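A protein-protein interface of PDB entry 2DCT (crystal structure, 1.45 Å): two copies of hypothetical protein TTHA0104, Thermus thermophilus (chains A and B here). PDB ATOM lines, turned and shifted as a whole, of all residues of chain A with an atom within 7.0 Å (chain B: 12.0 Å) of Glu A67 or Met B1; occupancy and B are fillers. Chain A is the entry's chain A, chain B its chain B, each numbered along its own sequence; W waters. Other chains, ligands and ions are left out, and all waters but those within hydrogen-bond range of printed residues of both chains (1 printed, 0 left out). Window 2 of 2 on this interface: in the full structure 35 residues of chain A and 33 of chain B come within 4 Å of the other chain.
O of Val A62 touches CE of Met B1 (3.4 Å). Met B1 touches Val A64. Met B1 touches Glu A68 (CE to C, 3.7 Å). N of Ala A69 touches CE of Met B1, at 3.6 Å. Leu A70 touches Ile B3. Ile B3 touches Leu A71. Ala A76 touches Leu B6 (CB to CD2, 3.9 Å). Ala A76 touches Phe B23. Phe B23 touches Ala A77 (CZ to N, 3.9 Å). CE2 of Phe A78 touches O of Gln B24 (3.4 Å).
OE1 of Glu A67 sits at hydrogen-bond distance from N of Met B1 (2.5 Å). N of Ala A76 lies within hydrogen-bond range of O of Lys B4, at 2.8 Å. The backbone carbonyl oxygen of Glu B2 sits at hydrogen-bond distance from the backbone NH of Phe A78 (2.8 Å).
No position is printed for both chains. Of the 18 pairs that touch across the chains among the printed residues, none has its exchanged pair printed and touching as well.
Of the 10 printed residues of chain B, 7 touch a printed residue of chain A. Hydrophobic or aromatic side chains of chain B that line the printed part of chain A: Met B1, Ile B3, Leu B6 and Phe B23. Of the 15 printed residues of chain A, 10 touch a printed residue of chain B. Hydrophobic or aromatic side chains of chain A within 4 Å of the printed part of chain B: Val A62, Val A64, Ala A69, Leu A71, Ala A76 and Phe A78. Among the printed residues, 18 pairs touch across the chains. Among the printed residues, no Asp or Glu carboxylate lies within 4 Å of a Lys or Arg side-chain nitrogen of the other chain.
Arg A63 touches none of the printed residues of chain B. Val A64 touches just one residue of chain B: Met B1. No residue of chain B comes within 4 Å of Gly A65. Glu A66 touches none of the printed residues of chain B. Of chain B, only Met B1 (2.5 Å) comes within 4 Å of Glu A67. Of chain B, only Met B1 comes within 4 Å of Glu A68. Ala A69 touches just these residues of chain B: Met B1 (3.6 Å) and Ile B3 (3.7 Å). Of chain B, only Glu B2 and Phe B23 come within 4 Å of Ala A77. Of the printed residues of chain B, Phe A78 touches Glu B2 (2.8 Å), Phe B23 (3.5 Å) and Gln B24 (3.4 Å). Printed residues of chain A within 4 Å of Met B1: Val A62 (3.4 Å), Val A64 (3.8 Å), Glu A67 (2.5 Å), Glu A68 (3.7 Å) and Ala A69 (3.6 Å). Printed residues of chain A within 4 Å of Glu B2: Ala A76 (3.99 Å), Ala A77 (3.3 Å) and Phe A78 (2.8 Å). Printed residues of chain A within 4 Å of Leu B6: Ala A76. The nearest residue of chain A that does not touch Met B1 is Ala A77 (4.2 Å). The nearest printed residue of chain A that does not touch Lys B4 is Ala A77 (5.1 Å).
N of Val A62 is in hydrogen-bond range of O of Ala A69. The side-chain amino group of Lys B4 lies within salt-bridge range of the side-chain carboxylate of Glu B2, 3.98 Å away. The side-chain amino group (NZ) of Lys B4 sits at hydrogen-bond distance from the backbone carbonyl oxygen (O) of Val B22 (2.7 Å).
Water W1 lies within hydrogen-bond range of O of Phe A78 (2.6 Å) and N of Glu B2 (2.9 Å).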
ATOM      1  N   VAL A  62     -20.081  25.018  32.419  1.00  0.00           N
ATOM      2  CA  VAL A  62     -21.108  24.007  32.344  1.00  0.00           C
ATOM      3  C   VAL A  62     -20.798  23.040  31.232  1.00  0.00           C
ATOM      4  O   VAL A  62     -20.427  23.433  30.127  1.00  0.00           O
ATOM      5  CB  VAL A  62     -22.507  24.624  32.103  1.00  0.00           C
ATOM      6  CG1 VAL A  62     -22.517  25.445  30.823  1.00  0.00           C
ATOM      7  CG2 VAL A  62     -23.543  23.520  32.024  1.00  0.00           C
ATOM      8  N   ARG A  63     -20.917  21.761  31.544  1.00  0.00           N
ATOM      9  CA  ARG A  63     -20.698  20.752  30.544  1.00  0.00           C
ATOM     10  C   ARG A  63     -22.034  20.117  30.249  1.00  0.00           C
ATOM     11  O   ARG A  63     -22.761  19.737  31.163  1.00  0.00           O
ATOM     12  CB  ARG A  63     -19.755  19.659  31.026  1.00  0.00           C
ATOM     13  CG  ARG A  63     -19.628  18.591  29.965  1.00  0.00           C
ATOM     14  CD  ARG A  63     -19.138  17.270  30.478  1.00  0.00           C
ATOM     15  NE  ARG A  63     -19.328  16.260  29.443  1.00  0.00           N
ATOM     16  CZ  ARG A  63     -18.883  15.014  29.521  1.00  0.00           C
ATOM     17  NH1 ARG A  63     -18.212  14.611  30.592  1.00  0.00           N
ATOM     18  NH2 ARG A  63     -19.107  14.174  28.521  1.00  0.00           N
ATOM     19  N   VAL A  64     -22.368  20.040  28.971  1.00  0.00           N
ATOM     20  CA  VAL A  64     -23.587  19.385  28.541  1.00  0.00           C
ATOM     21  C   VAL A  64     -23.165  18.601  27.324  1.00  0.00           C
ATOM     22  O   VAL A  64     -22.772  19.173  26.311  1.00  0.00           O
ATOM     23  CB  VAL A  64     -24.695  20.360  28.129  1.00  0.00           C
ATOM     24  CG1 VAL A  64     -25.890  19.569  27.619  1.00  0.00           C
ATOM     25  CG2 VAL A  64     -25.104  21.218  29.313  1.00  0.00           C
ATOM     26  N   GLY A  65     -23.210  17.284  27.442  1.00  0.00           N
ATOM     27  CA  GLY A  65     -22.820  16.457  26.323  1.00  0.00           C
ATOM     28  C   GLY A  65     -21.365  16.655  25.963  1.00  0.00           C
ATOM     29  O   GLY A  65     -20.486  16.633  26.823  1.00  0.00           O
ATOM     30  N   GLU A  66     -21.117  16.865  24.679  1.00  0.00           N
ATOM     31  CA  GLU A  66     -19.766  17.039  24.172  1.00  0.00           C
ATOM     32  C   GLU A  66     -19.271  18.466  24.284  1.00  0.00           C
ATOM     33  O   GLU A  66     -18.175  18.790  23.828  1.00  0.00           O
ATOM     34  CB  GLU A  66     -19.718  16.614  22.708  1.00  0.00           C
ATOM     35  CG  GLU A  66     -20.110  15.173  22.470  1.00  0.00           C
ATOM     36  CD  GLU A  66     -20.177  14.836  20.997  1.00  0.00           C
ATOM     37  OE1 GLU A  66     -21.258  15.006  20.392  1.00  0.00           O
ATOM     38  OE2 GLU A  66     -19.144  14.413  20.442  1.00  0.00           O
ATOM     39  N   GLU A  67     -20.066  19.327  24.901  1.00  0.00           N
ATOM     40  CA  GLU A  67     -19.664  20.714  24.998  1.00  0.00           C
ATOM     41  C   GLU A  67     -19.580  21.271  26.398  1.00  0.00           C
ATOM     42  O   GLU A  67     -20.219  20.786  27.327  1.00  0.00           O
ATOM     43  CB  GLU A  67     -20.621  21.576  24.178  1.00  0.00           C
ATOM     44  CG  GLU A  67     -20.650  21.208  22.708  1.00  0.00           C
ATOM     45  CD  GLU A  67     -21.733  21.933  21.949  1.00  0.00           C
ATOM     46  OE1 GLU A  67     -22.922  21.689  22.240  1.00  0.00           O
ATOM     47  OE2 GLU A  67     -21.398  22.745  21.061  1.00  0.00           O
ATOM     48  N   GLU A  68     -18.750  22.295  26.527  1.00  0.00           N
ATOM     49  CA  GLU A  68     -18.574  23.010  27.772  1.00  0.00           C
ATOM     50  C   GLU A  68     -18.682  24.468  27.375  1.00  0.00           C
ATOM     51  O   GLU A  68     -18.214  24.870  26.313  1.00  0.00           O
ATOM     52  CB  GLU A  68     -17.203  22.746  28.395  1.00  0.00           C
ATOM     53  CG  GLU A  68     -17.077  21.411  29.102  1.00  0.00           C
ATOM     54  CD  GLU A  68     -15.903  21.384  30.061  1.00  0.00           C
ATOM     55  OE1 GLU A  68     -14.774  21.682  29.623  1.00  0.00           O
ATOM     56  OE2 GLU A  68     -16.111  21.071  31.253  1.00  0.00           O
ATOM     57  N   ALA A  69     -19.324  25.256  28.215  1.00  0.00           N
ATOM     58  CA  ALA A  69     -19.475  26.665  27.929  1.00  0.00           C
ATOM     59  C   ALA A  69     -19.444  27.383  29.251  1.00  0.00           C
ATOM     60  O   ALA A  69     -19.676  26.779  30.297  1.00  0.00           O
ATOM     61  CB  ALA A  69     -20.794  26.923  27.218  1.00  0.00           C
ATOM     62  N   LEU A  70     -19.139  28.669  29.206  1.00  0.00           N
ATOM     63  CA  LEU A  70     -19.106  29.446  30.422  1.00  0.00           C
ATOM     64  C   LEU A  70     -20.521  29.911  30.683  1.00  0.00           C
ATOM     65  O   LEU A  70     -21.123  30.610  29.865  1.00  0.00           O
ATOM     66  CB  LEU A  70     -18.182  30.653  30.279  1.00  0.00           C
ATOM     67  CG  LEU A  70     -18.109  31.536  31.526  1.00  0.00           C
ATOM     68  CD1 LEU A  70     -17.609  30.721  32.710  1.00  0.00           C
ATOM     69  CD2 LEU A  70     -17.185  32.714  31.263  1.00  0.00           C
ATOM     70  N   LEU A  71     -21.062  29.488  31.813  1.00  0.00           N
ATOM     71  CA  LEU A  71     -22.402  29.886  32.189  1.00  0.00           C
ATOM     72  C   LEU A  71     -22.215  31.104  33.072  1.00  0.00           C
ATOM     73  O   LEU A  71     -21.959  30.979  34.269  1.00  0.00           O
ATOM     74  CB  LEU A  71     -23.087  28.771  32.969  1.00  0.00           C
ATOM     75  CG  LEU A  71     -24.578  29.001  33.218  1.00  0.00           C
ATOM     76  CD1 LEU A  71     -25.348  28.864  31.909  1.00  0.00           C
ATOM     77  CD2 LEU A  71     -25.083  27.999  34.241  1.00  0.00           C
ATOM     78  N   ALA A  76     -28.546  30.606  31.004  1.00  0.00           N
ATOM     79  CA  ALA A  76     -29.105  29.319  31.356  1.00  0.00           C
ATOM     80  C   ALA A  76     -28.569  28.317  30.355  1.00  0.00           C
ATOM     81  O   ALA A  76     -28.358  28.648  29.188  1.00  0.00           O
ATOM     82  CB  ALA A  76     -30.614  29.365  31.290  1.00  0.00           C
ATOM     83  N   ALA A  77     -28.331  27.102  30.823  1.00  0.00           N
ATOM     84  CA  ALA A  77     -27.829  26.036  29.973  1.00  0.00           C
ATOM     85  C   ALA A  77     -28.751  24.855  30.170  1.00  0.00           C
ATOM     86  O   ALA A  77     -29.111  24.505  31.291  1.00  0.00           O
ATOM     87  CB  ALA A  77     -26.405  25.667  30.356  1.00  0.00           C
ATOM     88  N   PHE A  78     -29.110  24.234  29.062  1.00  0.00           N
ATOM     89  CA  PHE A  78     -30.028  23.116  29.059  1.00  0.00           C
ATOM     90  C   PHE A  78     -29.325  21.783  28.860  1.00  0.00           C
ATOM     91  O   PHE A  78     -28.592  21.596  27.895  1.00  0.00           O
ATOM     92  CB  PHE A  78     -31.054  23.383  27.954  1.00  0.00           C
ATOM     93  CG  PHE A  78     -32.032  22.278  27.726  1.00  0.00           C
ATOM     94  CD1 PHE A  78     -32.669  21.647  28.786  1.00  0.00           C
ATOM     95  CD2 PHE A  78     -32.370  21.917  26.429  1.00  0.00           C
ATOM     96  CE1 PHE A  78     -33.630  20.667  28.550  1.00  0.00           C
ATOM     97  CE2 PHE A  78     -33.326  20.943  26.187  1.00  0.00           C
ATOM     98  CZ  PHE A  78     -33.959  20.317  27.250  1.00  0.00           C
ATOM     99  N   PRO A  84     -24.595  13.862  29.482  1.00  0.00           N
ATOM    100  CA  PRO A  84     -23.795  13.975  30.697  1.00  0.00           C
ATOM    101  C   PRO A  84     -23.676  15.467  30.934  1.00  0.00           C
ATOM    102  O   PRO A  84     -23.543  16.251  29.993  1.00  0.00           O
ATOM    103  CB  PRO A  84     -22.469  13.334  30.305  1.00  0.00           C
ATOM    104  CG  PRO A  84     -22.392  13.592  28.829  1.00  0.00           C
ATOM    105  CD  PRO A  84     -23.800  13.317  28.370  1.00  0.00           C
ATOM    106  N   GLY A  86     -22.521  18.681  33.989  1.00  0.00           N
ATOM    107  CA  GLY A  86     -21.937  19.022  35.255  1.00  0.00           C
ATOM    108  C   GLY A  86     -21.605  20.480  35.174  1.00  0.00           C
ATOM    109  O   GLY A  86     -21.732  21.109  34.125  1.00  0.00           O
ATOM    110  N   MET B   1     -24.239  23.733  22.678  1.00  0.00           N
ATOM    111  CA  MET B   1     -25.325  23.338  23.617  1.00  0.00           C
ATOM    112  C   MET B   1     -26.347  24.454  23.662  1.00  0.00           C
ATOM    113  O   MET B   1     -26.094  25.558  23.181  1.00  0.00           O
ATOM    114  CB  MET B   1     -24.769  23.130  25.031  1.00  0.00           C
ATOM    115  CG  MET B   1     -24.286  24.417  25.696  1.00  0.00           C
ATOM    116  SD  MET B   1     -23.788  24.228  27.423  1.00  0.00           S
ATOM    117  CE  MET B   1     -22.230  23.393  27.213  1.00  0.00           C
ATOM    118  N   GLU B   2     -27.508  24.160  24.232  1.00  0.00           N
ATOM    119  CA  GLU B   2     -28.543  25.167  24.376  1.00  0.00           C
ATOM    120  C   GLU B   2     -28.138  25.979  25.597  1.00  0.00           C
ATOM    121  O   GLU B   2     -28.237  25.507  26.727  1.00  0.00           O
ATOM    122  CB  GLU B   2     -29.902  24.512  24.616  1.00  0.00           C
ATOM    123  CG  GLU B   2     -30.551  23.935  23.372  1.00  0.00           C
ATOM    124  CD  GLU B   2     -30.776  24.988  22.307  1.00  0.00           C
ATOM    125  OE1 GLU B   2     -29.899  25.145  21.431  1.00  0.00           O
ATOM    126  OE2 GLU B   2     -31.822  25.668  22.359  1.00  0.00           O
ATOM    127  N   ILE B   3     -27.644  27.187  25.358  1.00  0.00           N
ATOM    128  CA  ILE B   3     -27.215  28.071  26.431  1.00  0.00           C
ATOM    129  C   ILE B   3     -27.554  29.478  25.971  1.00  0.00           C
ATOM    130  O   ILE B   3     -27.089  29.938  24.925  1.00  0.00           O
ATOM    131  CB  ILE B   3     -25.702  27.905  26.710  1.00  0.00           C
ATOM    132  CG1 ILE B   3     -25.255  28.891  27.786  1.00  0.00           C
ATOM    133  CG2 ILE B   3     -24.910  28.063  25.427  1.00  0.00           C
ATOM    134  CD1 ILE B   3     -23.851  28.632  28.288  1.00  0.00           C
ATOM    135  N   LYS B   4     -28.387  30.156  26.750  1.00  0.00           N
ATOM    136  CA  LYS B   4     -28.838  31.483  26.372  1.00  0.00           C
ATOM    137  C   LYS B   4     -28.829  32.510  27.481  1.00  0.00           C
ATOM    138  O   LYS B   4     -28.897  32.179  28.662  1.00  0.00           O
ATOM    139  CB  LYS B   4     -30.261  31.392  25.827  1.00  0.00           C
ATOM    140  CG  LYS B   4     -30.452  30.344  24.752  1.00  0.00           C
ATOM    141  CD  LYS B   4     -31.893  30.297  24.302  1.00  0.00           C
ATOM    142  CE  LYS B   4     -32.089  29.269  23.205  1.00  0.00           C
ATOM    143  NZ  LYS B   4     -33.496  29.255  22.725  1.00  0.00           N
ATOM    144  N   ASP B   5     -28.742  33.768  27.070  1.00  0.00           N
ATOM    145  CA  ASP B   5     -28.783  34.890  27.987  1.00  0.00           C
ATOM    146  C   ASP B   5     -30.274  35.189  28.026  1.00  0.00           C
ATOM    147  O   ASP B   5     -30.842  35.690  27.058  1.00  0.00           O
ATOM    148  CB  ASP B   5     -28.022  36.077  27.406  1.00  0.00           C
ATOM    149  CG  ASP B   5     -28.023  37.271  28.329  1.00  0.00           C
ATOM    150  OD1 ASP B   5     -29.123  37.716  28.718  1.00  0.00           O
ATOM    151  OD2 ASP B   5     -26.925  37.763  28.660  1.00  0.00           O
ATOM    152  N   LEU B   6     -30.911  34.875  29.146  1.00  0.00           N
ATOM    153  CA  LEU B   6     -32.348  35.058  29.271  1.00  0.00           C
ATOM    154  C   LEU B   6     -32.908  36.436  28.954  1.00  0.00           C
ATOM    155  O   LEU B   6     -33.795  36.568  28.113  1.00  0.00           O
ATOM    156  CB  LEU B   6     -32.801  34.636  30.668  1.00  0.00           C
ATOM    157  CG  LEU B   6     -32.448  33.194  31.043  1.00  0.00           C
ATOM    158  CD1 LEU B   6     -33.151  32.833  32.335  1.00  0.00           C
ATOM    159  CD2 LEU B   6     -32.863  32.241  29.929  1.00  0.00           C
ATOM    160  N   LEU B   9     -33.493  37.554  25.487  1.00  0.00           N
ATOM    161  CA  LEU B   9     -34.574  36.883  24.772  1.00  0.00           C
ATOM    162  C   LEU B   9     -35.914  37.568  25.007  1.00  0.00           C
ATOM    163  O   LEU B   9     -36.867  37.357  24.263  1.00  0.00           O
ATOM    164  CB  LEU B   9     -34.688  35.428  25.228  1.00  0.00           C
ATOM    165  CG  LEU B   9     -33.498  34.500  24.996  1.00  0.00           C
ATOM    166  CD1 LEU B   9     -33.762  33.167  25.682  1.00  0.00           C
ATOM    167  CD2 LEU B   9     -33.278  34.307  23.505  1.00  0.00           C
ATOM    168  N   VAL B  22     -37.636  29.615  26.347  1.00  0.00           N
ATOM    169  CA  VAL B  22     -36.186  29.695  26.413  1.00  0.00           C
ATOM    170  C   VAL B  22     -35.604  28.423  25.834  1.00  0.00           C
ATOM    171  O   VAL B  22     -34.799  28.458  24.907  1.00  0.00           O
ATOM    172  CB  VAL B  22     -35.705  29.851  27.858  1.00  0.00           C
ATOM    173  CG1 VAL B  22     -34.186  29.845  27.903  1.00  0.00           C
ATOM    174  CG2 VAL B  22     -36.260  31.135  28.437  1.00  0.00           C
ATOM    175  N   PHE B  23     -36.014  27.296  26.397  1.00  0.00           N
ATOM    176  CA  PHE B  23     -35.556  26.007  25.917  1.00  0.00           C
ATOM    177  C   PHE B  23     -36.770  25.198  25.547  1.00  0.00           C
ATOM    178  O   PHE B  23     -37.873  25.452  26.028  1.00  0.00           O
ATOM    179  CB  PHE B  23     -34.761  25.270  26.994  1.00  0.00           C
ATOM    180  CG  PHE B  23     -33.496  25.962  27.377  1.00  0.00           C
ATOM    181  CD1 PHE B  23     -32.504  26.184  26.430  1.00  0.00           C
ATOM    182  CD2 PHE B  23     -33.302  26.419  28.673  1.00  0.00           C
ATOM    183  CE1 PHE B  23     -31.335  26.853  26.768  1.00  0.00           C
ATOM    184  CE2 PHE B  23     -32.140  27.088  29.022  1.00  0.00           C
ATOM    185  CZ  PHE B  23     -31.154  27.306  28.069  1.00  0.00           C
ATOM    186  N   GLN B  24     -36.565  24.240  24.659  1.00  0.00           N
ATOM    187  CA  GLN B  24     -37.633  23.368  24.232  1.00  0.00           C
ATOM    188  C   GLN B  24     -37.328  22.071  24.946  1.00  0.00           C
ATOM    189  O   GLN B  24     -36.349  21.398  24.638  1.00  0.00           O
ATOM    190  CB  GLN B  24     -37.588  23.173  22.721  1.00  0.00           C
ATOM    191  CG  GLN B  24     -38.835  22.524  22.161  1.00  0.00           C
ATOM    192  CD  GLN B  24     -38.795  22.404  20.653  1.00  0.00           C
ATOM    193  OE1 GLN B  24     -38.241  21.451  20.109  1.00  0.00           O
ATOM    194  NE2 GLN B  24     -39.377  23.379  19.967  1.00  0.00           N
HETATM  195  O   HOH W   1     -28.339  21.635  25.298  1.00  0.00           O
